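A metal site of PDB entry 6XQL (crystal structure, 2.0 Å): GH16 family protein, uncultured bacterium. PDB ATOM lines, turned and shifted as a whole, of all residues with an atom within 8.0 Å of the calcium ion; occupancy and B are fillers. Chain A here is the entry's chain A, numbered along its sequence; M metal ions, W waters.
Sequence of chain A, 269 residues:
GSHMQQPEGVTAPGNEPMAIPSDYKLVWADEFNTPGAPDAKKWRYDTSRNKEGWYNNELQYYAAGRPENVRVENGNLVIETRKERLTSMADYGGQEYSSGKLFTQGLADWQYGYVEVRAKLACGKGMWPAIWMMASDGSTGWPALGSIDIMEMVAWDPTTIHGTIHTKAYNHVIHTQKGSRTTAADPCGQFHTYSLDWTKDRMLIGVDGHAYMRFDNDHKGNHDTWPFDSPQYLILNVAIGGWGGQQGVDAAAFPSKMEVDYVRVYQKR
Water W1 binds the calcium ion (2.3 Å). O of Gly 75 is bound to the calcium ion. O of Glu 31 is bound to the calcium ion. The calcium ion is bound by O of Asp 261, 2.4 Å away. The calcium ion is bound by the side-chain carboxylate (OD1) of Asp 261 (2.4 Å). Water W3 binds the calcium ion (2.6 Å). The calcium ion is bound by water W2 (2.6 Å).
NE of Arg 264 is in salt-bridge range of OE2 of Glu 31 (2.9 Å). The side-chain carboxylate (OD2) of Asp 261 lies within salt-bridge range of the guanidinium group (NH1) of Arg 118 (2.8 Å).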
ATOM      1  N   ASP A  30       2.174  17.649   7.679  1.00  0.00           N
ATOM      2  CA  ASP A  30       1.843  16.961   6.414  1.00  0.00           C
ATOM      3  C   ASP A  30       1.209  15.652   6.833  1.00  0.00           C
ATOM      4  O   ASP A  30       1.930  14.785   7.405  1.00  0.00           O
ATOM      5  CB  ASP A  30       3.063  16.816   5.524  1.00  0.00           C
ATOM      6  CG  ASP A  30       2.607  16.529   4.103  1.00  0.00           C
ATOM      7  OD1 ASP A  30       1.393  16.237   3.935  1.00  0.00           O
ATOM      8  OD2 ASP A  30       3.462  16.621   3.175  1.00  0.00           O
ATOM      9  N   GLU A  31      -0.102  15.574   6.624  1.00  0.00           N
ATOM     10  CA  GLU A  31      -0.936  14.378   6.847  1.00  0.00           C
ATOM     11  C   GLU A  31      -0.788  13.434   5.660  1.00  0.00           C
ATOM     12  O   GLU A  31      -1.248  12.307   5.772  1.00  0.00           O
ATOM     13  CB  GLU A  31      -2.387  14.812   7.038  1.00  0.00           C
ATOM     14  CG  GLU A  31      -2.546  15.695   8.249  1.00  0.00           C
ATOM     15  CD  GLU A  31      -2.319  15.062   9.617  1.00  0.00           C
ATOM     16  OE1 GLU A  31      -2.131  13.796   9.753  1.00  0.00           O
ATOM     17  OE2 GLU A  31      -2.385  15.838  10.568  1.00  0.00           O
ATOM     18  N   PHE A  32      -0.180  13.903   4.567  1.00  0.00           N
ATOM     19  CA  PHE A  32       0.040  13.121   3.327  1.00  0.00           C
ATOM     20  C   PHE A  32      -1.318  12.636   2.842  1.00  0.00           C
ATOM     21  O   PHE A  32      -1.441  11.496   2.367  1.00  0.00           O
ATOM     22  CB  PHE A  32       1.046  11.984   3.547  1.00  0.00           C
ATOM     23  CG  PHE A  32       2.397  12.487   3.985  1.00  0.00           C
ATOM     24  CD1 PHE A  32       3.167  13.300   3.152  1.00  0.00           C
ATOM     25  CD2 PHE A  32       2.868  12.205   5.255  1.00  0.00           C
ATOM     26  CE1 PHE A  32       4.367  13.833   3.595  1.00  0.00           C
ATOM     27  CE2 PHE A  32       4.080  12.714   5.671  1.00  0.00           C
ATOM     28  CZ  PHE A  32       4.831  13.526   4.846  1.00  0.00           C
ATOM     29  N   ASN A  33      -2.304  13.533   2.847  1.00  0.00           N
ATOM     30  CA  ASN A  33      -3.667  13.232   2.362  1.00  0.00           C
ATOM     31  C   ASN A  33      -3.726  13.158   0.837  1.00  0.00           C
ATOM     32  O   ASN A  33      -4.639  12.526   0.327  1.00  0.00           O
ATOM     33  CB  ASN A  33      -4.700  14.272   2.823  1.00  0.00           C
ATOM     34  CG  ASN A  33      -4.821  14.399   4.329  1.00  0.00           C
ATOM     35  OD1 ASN A  33      -4.626  13.443   5.089  1.00  0.00           O
ATOM     36  ND2 ASN A  33      -5.214  15.584   4.754  1.00  0.00           N
ATOM     37  N   THR A  34      -2.854  13.847   0.119  1.00  0.00           N
ATOM     38  CA  THR A  34      -2.968  14.004  -1.341  1.00  0.00           C
ATOM     39  C   THR A  34      -2.068  13.013  -2.052  1.00  0.00           C
ATOM     40  O   THR A  34      -0.849  13.117  -2.016  1.00  0.00           O
ATOM     41  CB  THR A  34      -2.613  15.432  -1.780  1.00  0.00           C
ATOM     42  OG1 THR A  34      -3.382  16.260  -0.914  1.00  0.00           O
ATOM     43  CG2 THR A  34      -2.899  15.675  -3.236  1.00  0.00           C
ATOM     44  N   VAL A  72       3.284   9.835  -2.329  1.00  0.00           N
ATOM     45  CA  VAL A  72       2.213   9.868  -1.316  1.00  0.00           C
ATOM     46  C   VAL A  72       1.163   8.902  -1.836  1.00  0.00           C
ATOM     47  O   VAL A  72       0.717   9.009  -3.053  1.00  0.00           O
ATOM     48  CB  VAL A  72       1.690  11.311  -1.097  1.00  0.00           C
ATOM     49  CG1 VAL A  72       0.536  11.331  -0.102  1.00  0.00           C
ATOM     50  CG2 VAL A  72       2.806  12.266  -0.655  1.00  0.00           C
ATOM     51  N   GLU A  73       0.828   7.944  -1.001  1.00  0.00           N
ATOM     52  CA  GLU A  73      -0.011   6.798  -1.406  1.00  0.00           C
ATOM     53  C   GLU A  73      -0.801   6.300  -0.205  1.00  0.00           C
ATOM     54  O   GLU A  73      -0.173   5.881   0.777  1.00  0.00           O
ATOM     55  CB  GLU A  73       0.976   5.775  -1.981  1.00  0.00           C
ATOM     56  CG  GLU A  73       0.383   4.677  -2.793  1.00  0.00           C
ATOM     57  CD  GLU A  73       1.432   3.621  -3.080  1.00  0.00           C
ATOM     58  OE1 GLU A  73       1.549   2.775  -2.240  1.00  0.00           O
ATOM     59  OE2 GLU A  73       2.134   3.692  -4.095  1.00  0.00           O
ATOM     60  N   ASN A  74      -2.134   6.343  -0.247  1.00  0.00           N
ATOM     61  CA  ASN A  74      -2.953   5.695   0.795  1.00  0.00           C
ATOM     62  C   ASN A  74      -2.681   6.324   2.151  1.00  0.00           C
ATOM     63  O   ASN A  74      -2.580   5.603   3.146  1.00  0.00           O
ATOM     64  CB  ASN A  74      -2.653   4.209   0.847  1.00  0.00           C
ATOM     65  CG  ASN A  74      -3.959   3.471   0.777  1.00  0.00           C
ATOM     66  OD1 ASN A  74      -4.543   3.175   1.831  1.00  0.00           O
ATOM     67  ND2 ASN A  74      -4.488   3.300  -0.447  1.00  0.00           N
ATOM     68  N   GLY A  75      -2.561   7.650   2.171  1.00  0.00           N
ATOM     69  CA  GLY A  75      -2.395   8.437   3.407  1.00  0.00           C
ATOM     70  C   GLY A  75      -0.968   8.517   3.908  1.00  0.00           C
ATOM     71  O   GLY A  75      -0.744   9.163   4.929  1.00  0.00           O
ATOM     72  N   ASN A  76      -0.023   7.868   3.247  1.00  0.00           N
ATOM     73  CA  ASN A  76       1.372   7.857   3.744  1.00  0.00           C
ATOM     74  C   ASN A  76       2.305   8.454   2.714  1.00  0.00           C
ATOM     75  O   ASN A  76       2.087   8.212   1.484  1.00  0.00           O
ATOM     76  CB  ASN A  76       1.874   6.448   4.062  1.00  0.00           C
ATOM     77  CG  ASN A  76       0.892   5.724   4.962  1.00  0.00           C
ATOM     78  OD1 ASN A  76       0.427   6.299   5.930  1.00  0.00           O
ATOM     79  ND2 ASN A  76       0.585   4.494   4.617  1.00  0.00           N
ATOM     80  N   LEU A  77       3.314   9.169   3.199  1.00  0.00           N
ATOM     81  CA  LEU A  77       4.543   9.323   2.402  1.00  0.00           C
ATOM     82  C   LEU A  77       5.210   7.965   2.302  1.00  0.00           C
ATOM     83  O   LEU A  77       5.486   7.378   3.365  1.00  0.00           O
ATOM     84  CB  LEU A  77       5.532  10.264   3.064  1.00  0.00           C
ATOM     85  CG  LEU A  77       6.793  10.498   2.243  1.00  0.00           C
ATOM     86  CD1 LEU A  77       6.462  11.205   0.916  1.00  0.00           C
ATOM     87  CD2 LEU A  77       7.757  11.301   3.077  1.00  0.00           C
ATOM     88  N   ARG A 118       4.453   9.742  12.693  1.00  0.00           N
ATOM     89  CA  ARG A 118       3.933   8.366  12.802  1.00  0.00           C
ATOM     90  C   ARG A 118       4.394   7.611  11.546  1.00  0.00           C
ATOM     91  O   ARG A 118       4.101   8.067  10.408  1.00  0.00           O
ATOM     92  CB  ARG A 118       2.417   8.321  12.995  1.00  0.00           C
ATOM     93  CG  ARG A 118       1.861   6.899  13.040  1.00  0.00           C
ATOM     94  CD  ARG A 118       0.416   6.948  13.525  1.00  0.00           C
ATOM     95  NE  ARG A 118      -0.106   5.630  13.847  1.00  0.00           N
ATOM     96  CZ  ARG A 118      -0.744   4.845  12.993  1.00  0.00           C
ATOM     97  NH1 ARG A 118      -0.951   5.236  11.744  1.00  0.00           N
ATOM     98  NH2 ARG A 118      -1.148   3.640  13.375  1.00  0.00           N
ATOM     99  N   PHE A 191       3.146   0.807  12.679  1.00  0.00           N
ATOM    100  CA  PHE A 191       3.406   2.246  12.891  1.00  0.00           C
ATOM    101  C   PHE A 191       3.709   2.525  14.360  1.00  0.00           C
ATOM    102  O   PHE A 191       3.061   1.937  15.242  1.00  0.00           O
ATOM    103  CB  PHE A 191       2.189   3.108  12.533  1.00  0.00           C
ATOM    104  CG  PHE A 191       1.991   3.242  11.050  1.00  0.00           C
ATOM    105  CD1 PHE A 191       2.773   4.138  10.331  1.00  0.00           C
ATOM    106  CD2 PHE A 191       1.030   2.481  10.386  1.00  0.00           C
ATOM    107  CE1 PHE A 191       2.609   4.267   8.961  1.00  0.00           C
ATOM    108  CE2 PHE A 191       0.889   2.607   9.017  1.00  0.00           C
ATOM    109  CZ  PHE A 191       1.690   3.492   8.320  1.00  0.00           C
ATOM    110  N   VAL A 260       5.381   7.105   6.100  1.00  0.00           N
ATOM    111  CA  VAL A 260       5.096   8.199   7.060  1.00  0.00           C
ATOM    112  C   VAL A 260       3.625   8.617   6.960  1.00  0.00           C
ATOM    113  O   VAL A 260       3.196   9.174   5.945  1.00  0.00           O
ATOM    114  CB  VAL A 260       6.035   9.393   6.886  1.00  0.00           C
ATOM    115  CG1 VAL A 260       5.842  10.378   8.040  1.00  0.00           C
ATOM    116  CG2 VAL A 260       7.490   8.968   6.756  1.00  0.00           C
ATOM    117  N   ASP A 261       2.886   8.314   8.004  1.00  0.00           N
ATOM    118  CA  ASP A 261       1.433   8.556   8.075  1.00  0.00           C
ATOM    119  C   ASP A 261       1.258  10.054   8.200  1.00  0.00           C
ATOM    120  O   ASP A 261       0.484  10.639   7.455  1.00  0.00           O
ATOM    121  CB  ASP A 261       0.843   7.781   9.225  1.00  0.00           C
ATOM    122  CG  ASP A 261      -0.601   8.133   9.457  1.00  0.00           C
ATOM    123  OD1 ASP A 261      -1.214   8.748   8.579  1.00  0.00           O
ATOM    124  OD2 ASP A 261      -1.086   7.737  10.485  1.00  0.00           O
ATOM    125  N   TYR A 262       2.028  10.671   9.078  1.00  0.00           N
ATOM    126  CA  TYR A 262       1.954  12.132   9.238  1.00  0.00           C
ATOM    127  C   TYR A 262       3.250  12.634   9.838  1.00  0.00           C
ATOM    128  O   TYR A 262       3.973  11.872  10.501  1.00  0.00           O
ATOM    129  CB  TYR A 262       0.710  12.481  10.052  1.00  0.00           C
ATOM    130  CG  TYR A 262       0.649  11.936  11.459  1.00  0.00           C
ATOM    131  CD1 TYR A 262       1.476  12.428  12.446  1.00  0.00           C
ATOM    132  CD2 TYR A 262      -0.279  10.975  11.836  1.00  0.00           C
ATOM    133  CE1 TYR A 262       1.405  11.966  13.753  1.00  0.00           C
ATOM    134  CE2 TYR A 262      -0.371  10.516  13.142  1.00  0.00           C
ATOM    135  CZ  TYR A 262       0.475  11.007  14.097  1.00  0.00           C
ATOM    136  OH  TYR A 262       0.434  10.555  15.397  1.00  0.00           O
ATOM    137  N   VAL A 263       3.491  13.906   9.564  1.00  0.00           N
ATOM    138  CA  VAL A 263       4.382  14.779  10.353  1.00  0.00           C
ATOM    139  C   VAL A 263       3.531  15.873  10.950  1.00  0.00           C
ATOM    140  O   VAL A 263       2.863  16.573  10.178  1.00  0.00           O
ATOM    141  CB  VAL A 263       5.484  15.422   9.508  1.00  0.00           C
ATOM    142  CG1 VAL A 263       6.349  16.325  10.368  1.00  0.00           C
ATOM    143  CG2 VAL A 263       6.309  14.367   8.822  1.00  0.00           C
ATOM    144  N   ARG A 264       3.639  16.069  12.252  1.00  0.00           N
ATOM    145  CA  ARG A 264       2.821  17.086  12.953  1.00  0.00           C
ATOM    146  C   ARG A 264       3.763  17.882  13.839  1.00  0.00           C
ATOM    147  O   ARG A 264       4.503  17.240  14.631  1.00  0.00           O
ATOM    148  CB  ARG A 264       1.721  16.419  13.775  1.00  0.00           C
ATOM    149  CG  ARG A 264       0.593  15.840  12.920  1.00  0.00           C
ATOM    150  CD  ARG A 264      -0.502  15.178  13.730  1.00  0.00           C
ATOM    151  NE  ARG A 264      -1.419  14.407  12.880  1.00  0.00           N
ATOM    152  CZ  ARG A 264      -2.167  13.395  13.301  1.00  0.00           C
ATOM    153  NH1 ARG A 264      -2.100  12.980  14.550  1.00  0.00           N
ATOM    154  NH2 ARG A 264      -2.957  12.769  12.451  1.00  0.00           N
HETATM  155 CA    CA M   1      -1.790  10.228   6.759  1.00  0.00          CA
HETATM  156  O   HOH W   1      -3.667  10.933   5.551  1.00  0.00           O
HETATM  157  O   HOH W   2      -3.755   8.478   6.712  1.00  0.00           O
HETATM  158  O   HOH W   3      -2.663  11.643   8.743  1.00  0.00           O
